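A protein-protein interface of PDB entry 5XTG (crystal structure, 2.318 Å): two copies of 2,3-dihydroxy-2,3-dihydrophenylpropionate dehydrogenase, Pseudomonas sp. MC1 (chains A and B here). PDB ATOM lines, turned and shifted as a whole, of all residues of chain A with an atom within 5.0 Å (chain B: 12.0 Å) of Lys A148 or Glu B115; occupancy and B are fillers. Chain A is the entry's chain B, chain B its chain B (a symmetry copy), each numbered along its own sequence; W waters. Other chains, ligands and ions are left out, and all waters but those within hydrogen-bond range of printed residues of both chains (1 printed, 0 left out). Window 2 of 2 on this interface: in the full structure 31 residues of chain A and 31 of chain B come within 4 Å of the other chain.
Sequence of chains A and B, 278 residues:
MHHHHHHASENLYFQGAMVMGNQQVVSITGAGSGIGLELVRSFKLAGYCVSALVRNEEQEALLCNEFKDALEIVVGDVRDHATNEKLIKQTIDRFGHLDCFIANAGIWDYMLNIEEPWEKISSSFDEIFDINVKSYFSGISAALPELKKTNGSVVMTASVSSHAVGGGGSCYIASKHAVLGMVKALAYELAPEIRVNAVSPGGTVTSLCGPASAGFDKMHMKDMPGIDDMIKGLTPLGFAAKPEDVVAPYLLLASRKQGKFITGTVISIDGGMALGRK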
ATOM      1  N   LEU A 144      32.548  -8.238  24.317  1.00  0.00           N
ATOM      2  CA  LEU A 144      32.505  -6.970  23.588  1.00  0.00           C
ATOM      3  C   LEU A 144      33.217  -5.829  24.301  1.00  0.00           C
ATOM      4  O   LEU A 144      34.020  -5.130  23.655  1.00  0.00           O
ATOM      5  CB  LEU A 144      31.045  -6.607  23.333  1.00  0.00           C
ATOM      6  CG  LEU A 144      30.790  -5.638  22.198  1.00  0.00           C
ATOM      7  CD1 LEU A 144      31.099  -6.338  20.945  1.00  0.00           C
ATOM      8  CD2 LEU A 144      29.330  -5.200  22.184  1.00  0.00           C
ATOM      9  N   PRO A 145      32.964  -5.561  25.589  1.00  0.00           N
ATOM     10  CA  PRO A 145      33.618  -4.406  26.223  1.00  0.00           C
ATOM     11  C   PRO A 145      35.109  -4.426  26.020  1.00  0.00           C
ATOM     12  O   PRO A 145      35.730  -3.393  25.737  1.00  0.00           O
ATOM     13  CB  PRO A 145      33.256  -4.566  27.697  1.00  0.00           C
ATOM     14  CG  PRO A 145      31.998  -5.471  27.680  1.00  0.00           C
ATOM     15  CD  PRO A 145      32.260  -6.407  26.570  1.00  0.00           C
ATOM     16  N   GLU A 146      35.695  -5.614  26.123  1.00  0.00           N
ATOM     17  CA  GLU A 146      37.136  -5.739  26.084  1.00  0.00           C
ATOM     18  C   GLU A 146      37.676  -5.686  24.659  1.00  0.00           C
ATOM     19  O   GLU A 146      38.769  -5.156  24.439  1.00  0.00           O
ATOM     20  CB  GLU A 146      37.530  -7.018  26.811  1.00  0.00           C
ATOM     21  CG  GLU A 146      37.117  -7.010  28.301  1.00  0.00           C
ATOM     22  CD  GLU A 146      37.781  -5.841  29.143  1.00  0.00           C
ATOM     23  OE1 GLU A 146      38.957  -5.481  28.872  1.00  0.00           O
ATOM     24  OE2 GLU A 146      37.137  -5.292  30.089  1.00  0.00           O
ATOM     25  N   LEU A 147      36.920  -6.181  23.676  1.00  0.00           N
ATOM     26  CA  LEU A 147      37.379  -6.052  22.304  1.00  0.00           C
ATOM     27  C   LEU A 147      37.299  -4.612  21.851  1.00  0.00           C
ATOM     28  O   LEU A 147      38.070  -4.197  20.980  1.00  0.00           O
ATOM     29  CB  LEU A 147      36.556  -6.928  21.367  1.00  0.00           C
ATOM     30  CG  LEU A 147      36.650  -8.431  21.575  1.00  0.00           C
ATOM     31  CD1 LEU A 147      35.633  -9.111  20.688  1.00  0.00           C
ATOM     32  CD2 LEU A 147      38.053  -8.925  21.271  1.00  0.00           C
ATOM     33  N   LYS A 148      36.362  -3.847  22.413  1.00  0.00           N
ATOM     34  CA  LYS A 148      36.246  -2.440  22.043  1.00  0.00           C
ATOM     35  C   LYS A 148      37.454  -1.638  22.507  1.00  0.00           C
ATOM     36  O   LYS A 148      37.805  -0.640  21.873  1.00  0.00           O
ATOM     37  CB  LYS A 148      34.973  -1.842  22.631  1.00  0.00           C
ATOM     38  CG  LYS A 148      33.792  -1.865  21.692  1.00  0.00           C
ATOM     39  CD  LYS A 148      32.557  -1.356  22.410  1.00  0.00           C
ATOM     40  CE  LYS A 148      31.394  -1.056  21.445  1.00  0.00           C
ATOM     41  NZ  LYS A 148      30.315  -0.252  22.174  1.00  0.00           N
ATOM     42  N   LYS A 149      38.104  -2.074  23.589  1.00  0.00           N
ATOM     43  CA  LYS A 149      39.292  -1.407  24.104  1.00  0.00           C
ATOM     44  C   LYS A 149      40.548  -1.699  23.305  1.00  0.00           C
ATOM     45  O   LYS A 149      41.555  -1.001  23.492  1.00  0.00           O
ATOM     46  CB  LYS A 149      39.575  -1.839  25.540  1.00  0.00           C
ATOM     47  CG  LYS A 149      38.663  -1.299  26.610  1.00  0.00           C
ATOM     48  CD  LYS A 149      39.140  -1.827  27.957  1.00  0.00           C
ATOM     49  CE  LYS A 149      38.000  -2.002  28.921  1.00  0.00           C
ATOM     50  NZ  LYS A 149      38.468  -2.496  30.255  1.00  0.00           N
ATOM     51  N   THR A 150      40.542  -2.751  22.487  1.00  0.00           N
ATOM     52  CA  THR A 150      41.680  -3.089  21.644  1.00  0.00           C
ATOM     53  C   THR A 150      41.371  -3.017  20.163  1.00  0.00           C
ATOM     54  O   THR A 150      42.245  -3.340  19.363  1.00  0.00           O
ATOM     55  CB  THR A 150      42.178  -4.514  21.948  1.00  0.00           C
ATOM     56  OG1 THR A 150      41.060  -5.419  21.982  1.00  0.00           O
ATOM     57  CG2 THR A 150      42.904  -4.579  23.268  1.00  0.00           C
ATOM     58  N   ASN A 151      40.158  -2.639  19.764  1.00  0.00           N
ATOM     59  CA  ASN A 151      39.737  -2.796  18.368  1.00  0.00           C
ATOM     60  C   ASN A 151      40.041  -4.215  17.862  1.00  0.00           C
ATOM     61  O   ASN A 151      40.673  -4.421  16.825  1.00  0.00           O
ATOM     62  CB  ASN A 151      40.398  -1.724  17.488  1.00  0.00           C
ATOM     63  CG  ASN A 151      39.811  -0.330  17.733  1.00  0.00           C
ATOM     64  OD1 ASN A 151      39.158  -0.073  18.749  1.00  0.00           O
ATOM     65  ND2 ASN A 151      40.022   0.560  16.787  1.00  0.00           N
ATOM     66  N   GLU A 189      27.321  -3.616  12.072  1.00  0.00           N
ATOM     67  CA  GLU A 189      27.021  -2.779  13.229  1.00  0.00           C
ATOM     68  C   GLU A 189      28.282  -2.378  13.995  1.00  0.00           C
ATOM     69  O   GLU A 189      28.364  -1.268  14.530  1.00  0.00           O
ATOM     70  CB  GLU A 189      26.043  -3.527  14.156  1.00  0.00           C
ATOM     71  CG  GLU A 189      26.056  -3.053  15.589  1.00  0.00           C
ATOM     72  CD  GLU A 189      24.977  -3.736  16.466  1.00  0.00           C
ATOM     73  OE1 GLU A 189      24.347  -4.746  16.026  1.00  0.00           O
ATOM     74  OE2 GLU A 189      24.770  -3.246  17.606  1.00  0.00           O
ATOM     75  N   LEU A 190      29.250  -3.276  14.108  1.00  0.00           N
ATOM     76  CA  LEU A 190      30.434  -3.027  14.921  1.00  0.00           C
ATOM     77  C   LEU A 190      31.590  -2.413  14.157  1.00  0.00           C
ATOM     78  O   LEU A 190      32.581  -2.012  14.776  1.00  0.00           O
ATOM     79  CB  LEU A 190      30.898  -4.330  15.545  1.00  0.00           C
ATOM     80  CG  LEU A 190      29.842  -4.912  16.474  1.00  0.00           C
ATOM     81  CD1 LEU A 190      30.343  -6.229  17.047  1.00  0.00           C
ATOM     82  CD2 LEU A 190      29.449  -3.939  17.592  1.00  0.00           C
ATOM     83  N   ILE A 194      35.484  -3.134  15.400  1.00  0.00           N
ATOM     84  CA  ILE A 194      35.568  -4.575  15.617  1.00  0.00           C
ATOM     85  C   ILE A 194      35.288  -5.313  14.309  1.00  0.00           C
ATOM     86  O   ILE A 194      34.243  -5.104  13.677  1.00  0.00           O
ATOM     87  CB  ILE A 194      34.609  -4.992  16.747  1.00  0.00           C
ATOM     88  CG1 ILE A 194      34.958  -4.176  18.016  1.00  0.00           C
ATOM     89  CG2 ILE A 194      34.707  -6.485  17.009  1.00  0.00           C
ATOM     90  CD1 ILE A 194      34.314  -4.593  19.242  1.00  0.00           C
ATOM     91  N   ASP B 109      12.734  -6.920  15.669  1.00  0.00           N
ATOM     92  CA  ASP B 109      13.584  -6.703  16.843  1.00  0.00           C
ATOM     93  C   ASP B 109      13.881  -5.229  17.112  1.00  0.00           C
ATOM     94  O   ASP B 109      14.644  -4.917  18.028  1.00  0.00           O
ATOM     95  CB  ASP B 109      14.898  -7.509  16.711  1.00  0.00           C
ATOM     96  CG  ASP B 109      15.912  -6.900  15.753  1.00  0.00           C
ATOM     97  OD1 ASP B 109      15.549  -6.009  14.944  1.00  0.00           O
ATOM     98  OD2 ASP B 109      17.090  -7.348  15.783  1.00  0.00           O
ATOM     99  N   TYR B 110      13.298  -4.304  16.353  1.00  0.00           N
ATOM    100  CA  TYR B 110      13.446  -2.878  16.667  1.00  0.00           C
ATOM    101  C   TYR B 110      14.920  -2.453  16.742  1.00  0.00           C
ATOM    102  O   TYR B 110      15.276  -1.528  17.461  1.00  0.00           O
ATOM    103  CB  TYR B 110      12.677  -2.545  17.961  1.00  0.00           C
ATOM    104  CG  TYR B 110      11.189  -2.682  17.736  1.00  0.00           C
ATOM    105  CD1 TYR B 110      10.435  -1.613  17.268  1.00  0.00           C
ATOM    106  CD2 TYR B 110      10.554  -3.894  17.904  1.00  0.00           C
ATOM    107  CE1 TYR B 110       9.082  -1.736  17.016  1.00  0.00           C
ATOM    108  CE2 TYR B 110       9.178  -4.031  17.654  1.00  0.00           C
ATOM    109  CZ  TYR B 110       8.454  -2.945  17.209  1.00  0.00           C
ATOM    110  OH  TYR B 110       7.097  -3.051  16.951  1.00  0.00           O
ATOM    111  N   MET B 111      15.783  -3.093  15.940  1.00  0.00           N
ATOM    112  CA  MET B 111      17.198  -2.715  15.784  1.00  0.00           C
ATOM    113  C   MET B 111      17.991  -2.886  17.074  1.00  0.00           C
ATOM    114  O   MET B 111      18.989  -2.194  17.296  1.00  0.00           O
ATOM    115  CB  MET B 111      17.366  -1.269  15.276  1.00  0.00           C
ATOM    116  CG  MET B 111      16.649  -0.908  13.959  1.00  0.00           C
ATOM    117  SD  MET B 111      17.083  -1.941  12.548  1.00  0.00           S
ATOM    118  CE  MET B 111      18.654  -1.210  12.046  1.00  0.00           C
ATOM    119  N   LEU B 112      17.567  -3.811  17.927  1.00  0.00           N
ATOM    120  CA  LEU B 112      18.240  -4.046  19.205  1.00  0.00           C
ATOM    121  C   LEU B 112      19.745  -4.238  19.027  1.00  0.00           C
ATOM    122  O   LEU B 112      20.188  -5.096  18.268  1.00  0.00           O
ATOM    123  CB  LEU B 112      17.625  -5.275  19.885  1.00  0.00           C
ATOM    124  CG  LEU B 112      18.139  -5.586  21.298  1.00  0.00           C
ATOM    125  CD1 LEU B 112      17.710  -4.497  22.196  1.00  0.00           C
ATOM    126  CD2 LEU B 112      17.614  -6.892  21.804  1.00  0.00           C
ATOM    127  N   ASN B 113      20.518  -3.447  19.766  1.00  0.00           N
ATOM    128  CA  ASN B 113      21.972  -3.374  19.636  1.00  0.00           C
ATOM    129  C   ASN B 113      22.637  -4.481  20.443  1.00  0.00           C
ATOM    130  O   ASN B 113      22.191  -4.814  21.549  1.00  0.00           O
ATOM    131  CB  ASN B 113      22.457  -2.005  20.136  1.00  0.00           C
ATOM    132  CG  ASN B 113      23.588  -1.450  19.321  1.00  0.00           C
ATOM    133  OD1 ASN B 113      24.746  -1.427  19.767  1.00  0.00           O
ATOM    134  ND2 ASN B 113      23.272  -0.993  18.109  1.00  0.00           N
ATOM    135  N   ILE B 114      23.715  -5.045  19.893  1.00  0.00           N
ATOM    136  CA  ILE B 114      24.480  -6.078  20.597  1.00  0.00           C
ATOM    137  C   ILE B 114      25.172  -5.545  21.849  1.00  0.00           C
ATOM    138  O   ILE B 114      25.655  -6.346  22.649  1.00  0.00           O
ATOM    139  CB  ILE B 114      25.521  -6.724  19.642  1.00  0.00           C
ATOM    140  CG1 ILE B 114      26.186  -7.983  20.244  1.00  0.00           C
ATOM    141  CG2 ILE B 114      26.614  -5.738  19.260  1.00  0.00           C
ATOM    142  CD1 ILE B 114      25.238  -9.189  20.373  1.00  0.00           C
ATOM    143  N   GLU B 115      25.234  -4.223  22.045  1.00  0.00           N
ATOM    144  CA  GLU B 115      25.876  -3.612  23.217  1.00  0.00           C
ATOM    145  C   GLU B 115      24.942  -3.504  24.417  1.00  0.00           C
ATOM    146  O   GLU B 115      25.365  -3.086  25.501  1.00  0.00           O
ATOM    147  CB  GLU B 115      26.407  -2.216  22.855  1.00  0.00           C
ATOM    148  CG  GLU B 115      27.664  -2.260  21.958  1.00  0.00           C
ATOM    149  CD  GLU B 115      27.730  -1.173  20.871  1.00  0.00           C
ATOM    150  OE1 GLU B 115      28.208  -1.482  19.746  1.00  0.00           O
ATOM    151  OE2 GLU B 115      27.323  -0.015  21.139  1.00  0.00           O
ATOM    152  N   GLU B 116      23.687  -3.846  24.233  1.00  0.00           N
ATOM    153  CA  GLU B 116      22.712  -3.806  25.297  1.00  0.00           C
ATOM    154  C   GLU B 116      22.971  -4.867  26.361  1.00  0.00           C
ATOM    155  O   GLU B 116      23.665  -5.860  26.117  1.00  0.00           O
ATOM    156  CB  GLU B 116      21.328  -4.038  24.717  1.00  0.00           C
ATOM    157  CG  GLU B 116      20.891  -2.942  23.793  1.00  0.00           C
ATOM    158  CD  GLU B 116      20.202  -1.769  24.514  1.00  0.00           C
ATOM    159  OE1 GLU B 116      19.667  -0.899  23.803  1.00  0.00           O
ATOM    160  OE2 GLU B 116      20.184  -1.698  25.774  1.00  0.00           O
ATOM    161  N   PRO B 117      22.381  -4.695  27.538  1.00  0.00           N
ATOM    162  CA  PRO B 117      22.513  -5.702  28.590  1.00  0.00           C
ATOM    163  C   PRO B 117      22.098  -7.072  28.088  1.00  0.00           C
ATOM    164  O   PRO B 117      21.066  -7.231  27.431  1.00  0.00           O
ATOM    165  CB  PRO B 117      21.560  -5.203  29.682  1.00  0.00           C
ATOM    166  CG  PRO B 117      21.455  -3.784  29.486  1.00  0.00           C
ATOM    167  CD  PRO B 117      21.562  -3.560  27.981  1.00  0.00           C
ATOM    168  N   TRP B 118      22.896  -8.071  28.460  1.00  0.00           N
ATOM    169  CA  TRP B 118      22.679  -9.420  27.963  1.00  0.00           C
ATOM    170  C   TRP B 118      21.262  -9.899  28.225  1.00  0.00           C
ATOM    171  O   TRP B 118      20.643 -10.526  27.362  1.00  0.00           O
ATOM    172  CB  TRP B 118      23.670 -10.398  28.582  1.00  0.00           C
ATOM    173  CG  TRP B 118      23.263 -11.777  28.222  1.00  0.00           C
ATOM    174  CD1 TRP B 118      22.808 -12.765  29.055  1.00  0.00           C
ATOM    175  CD2 TRP B 118      23.220 -12.313  26.911  1.00  0.00           C
ATOM    176  NE1 TRP B 118      22.510 -13.884  28.342  1.00  0.00           N
ATOM    177  CE2 TRP B 118      22.744 -13.633  27.020  1.00  0.00           C
ATOM    178  CE3 TRP B 118      23.543 -11.799  25.639  1.00  0.00           C
ATOM    179  CZ2 TRP B 118      22.584 -14.445  25.925  1.00  0.00           C
ATOM    180  CZ3 TRP B 118      23.380 -12.600  24.552  1.00  0.00           C
ATOM    181  CH2 TRP B 118      22.909 -13.915  24.695  1.00  0.00           C
ATOM    182  N   GLU B 119      20.729  -9.630  29.416  1.00  0.00           N
ATOM    183  CA  GLU B 119      19.398 -10.151  29.742  1.00  0.00           C
ATOM    184  C   GLU B 119      18.360  -9.542  28.839  1.00  0.00           C
ATOM    185  O   GLU B 119      17.335 -10.167  28.542  1.00  0.00           O
ATOM    186  CB  GLU B 119      19.042  -9.875  31.207  1.00  0.00           C
ATOM    187  CG  GLU B 119      19.785 -10.791  32.190  1.00  0.00           C
ATOM    188  CD  GLU B 119      19.484 -12.297  31.973  1.00  0.00           C
ATOM    189  OE1 GLU B 119      18.439 -12.640  31.343  1.00  0.00           O
ATOM    190  OE2 GLU B 119      20.303 -13.137  32.432  1.00  0.00           O
ATOM    191  N   LYS B 120      18.599  -8.321  28.394  1.00  0.00           N
ATOM    192  CA  LYS B 120      17.677  -7.751  27.438  1.00  0.00           C
ATOM    193  C   LYS B 120      17.822  -8.435  26.084  1.00  0.00           C
ATOM    194  O   LYS B 120      16.819  -8.703  25.419  1.00  0.00           O
ATOM    195  CB  LYS B 120      17.893  -6.246  27.333  1.00  0.00           C
ATOM    196  CG  LYS B 120      16.979  -5.592  26.295  1.00  0.00           C
ATOM    197  CD  LYS B 120      17.422  -4.176  25.897  1.00  0.00           C
ATOM    198  CE  LYS B 120      17.028  -3.117  26.912  1.00  0.00           C
ATOM    199  NZ  LYS B 120      17.335  -1.704  26.432  1.00  0.00           N
ATOM    200  N   ILE B 121      19.054  -8.748  25.668  1.00  0.00           N
ATOM    201  CA  ILE B 121      19.255  -9.414  24.375  1.00  0.00           C
ATOM    202  C   ILE B 121      18.646 -10.794  24.428  1.00  0.00           C
ATOM    203  O   ILE B 121      17.967 -11.241  23.499  1.00  0.00           O
ATOM    204  CB  ILE B 121      20.748  -9.493  24.031  1.00  0.00           C
ATOM    205  CG1 ILE B 121      21.349  -8.091  23.895  1.00  0.00           C
ATOM    206  CG2 ILE B 121      20.961 -10.280  22.720  1.00  0.00           C
ATOM    207  CD1 ILE B 121      22.840  -8.125  23.685  1.00  0.00           C
ATOM    208  N   SER B 122      18.832 -11.455  25.555  1.00  0.00           N
ATOM    209  CA  SER B 122      18.459 -12.846  25.700  1.00  0.00           C
ATOM    210  C   SER B 122      16.951 -13.022  25.637  1.00  0.00           C
ATOM    211  O   SER B 122      16.435 -13.917  24.952  1.00  0.00           O
ATOM    212  CB  SER B 122      19.008 -13.350  27.030  1.00  0.00           C
ATOM    213  OG  SER B 122      18.404 -14.570  27.385  1.00  0.00           O
ATOM    214  N   SER B 124      14.830 -11.018  24.225  1.00  0.00           N
ATOM    215  CA  SER B 124      14.389 -10.703  22.867  1.00  0.00           C
ATOM    216  C   SER B 124      14.733 -11.821  21.892  1.00  0.00           C
ATOM    217  O   SER B 124      13.924 -12.200  21.034  1.00  0.00           O
ATOM    218  CB  SER B 124      15.044  -9.405  22.414  1.00  0.00           C
ATOM    219  OG  SER B 124      15.001  -8.461  23.482  1.00  0.00           O
ATOM    220  N   GLY B 168      17.282  -4.412  10.278  1.00  0.00           N
ATOM    221  CA  GLY B 168      17.015  -5.020  11.574  1.00  0.00           C
ATOM    222  C   GLY B 168      18.297  -5.161  12.367  1.00  0.00           C
ATOM    223  O   GLY B 168      19.394  -4.955  11.861  1.00  0.00           O
ATOM    224  N   GLY B 169      18.147  -5.531  13.629  1.00  0.00           N
ATOM    225  CA  GLY B 169      19.290  -5.883  14.445  1.00  0.00           C
ATOM    226  C   GLY B 169      19.767  -7.289  14.154  1.00  0.00           C
ATOM    227  O   GLY B 169      19.169  -8.042  13.382  1.00  0.00           O
ATOM    228  N   SER B 170      20.867  -7.657  14.809  1.00  0.00           N
ATOM    229  CA  SER B 170      21.474  -8.954  14.539  1.00  0.00           C
ATOM    230  C   SER B 170      20.536 -10.116  14.860  1.00  0.00           C
ATOM    231  O   SER B 170      20.604 -11.153  14.192  1.00  0.00           O
ATOM    232  CB  SER B 170      22.761  -9.075  15.320  1.00  0.00           C
ATOM    233  OG  SER B 170      22.509  -8.859  16.695  1.00  0.00           O
ATOM    234  N   CYS B 171      19.653  -9.978  15.863  1.00  0.00           N
ATOM    235  CA  CYS B 171      18.719 -11.068  16.162  1.00  0.00           C
ATOM    236  C   CYS B 171      17.720 -11.252  15.034  1.00  0.00           C
ATOM    237  O   CYS B 171      17.420 -12.383  14.634  1.00  0.00           O
ATOM    238  CB  CYS B 171      17.965 -10.823  17.471  1.00  0.00           C
ATOM    239  SG  CYS B 171      18.936 -10.894  18.928  1.00  0.00           S
HETATM  240  O   HOH W   1      22.285  -6.239  16.809  1.00  0.00           O
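Leu A144 touches Ile B114 (CD2 to O, 3.9 Å). Glu B115 touches Leu A144. Leu A190 touches Ile B114 (CD2 to CG2, 3.7 Å). CD2 of Leu A190 touches OE1 of Glu B115 (3.5 Å).
OD1 of Asn B113 lies close to OE2 of Glu B115, 3.2 Å away. O of Lys A148 lies close to OD1 of Asn A151, at 3.5 Å.
No residue of chain B comes within 4 Å of Pro A145. No residue of chain B comes within 4 Å of Glu A146. No residue of chain B comes within 4 Å of Leu A147. No residue of chain B comes within 4 Å of Lys A149. No residue of chain B comes within 4 Å of Asn A151. Printed residues of chain B within 4 Å of Glu A189: Asn B113 and Ile B114. Of the printed residues of chain A, Asn B113 touches Glu A189. Of the printed residues of chain A, Ile B114 touches Leu A144 (3.9 Å), Glu A189 (3.1 Å) and Leu A190 (3.7 Å). Of chain A, only Leu A144 (3.4 Å), Lys A148 (3.0 Å) and Leu A190 (3.5 Å) come within 4 Å of Glu B115. The nearest printed residue of chain A that does not touch Asn B113 is Leu A190 (5.8 Å).
Of the 19 printed residues of chain B, 3 touch a printed residue of chain A. Hydrophobic or aromatic side chains of chain B that line the printed part of chain A: Ile B114. Among the printed residues, 7 pairs touch across the chains. Among the printed residues, Asp or Glu carboxylates within 4 Å of a Lys or Arg side-chain nitrogen of the other chain: Lys A148 with Glu B115 (3.2 Å).
Water W1 lies within hydrogen-bond range of OG of Ser B170 (2.6 Å), OE1 of Glu A189 (2.7 Å) and O of Leu B112 (2.8 Å).
ND2 of Asn B113 lies close to OE2 of Glu A189 (2.8 Å). NZ of Lys A148 lies within salt-bridge range of OE2 of Glu B115 (3.2 Å). OE2 of Glu A189 is in hydrogen-bond range of N of Ile B114, at 3.1 Å.
No position is printed for both chains.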
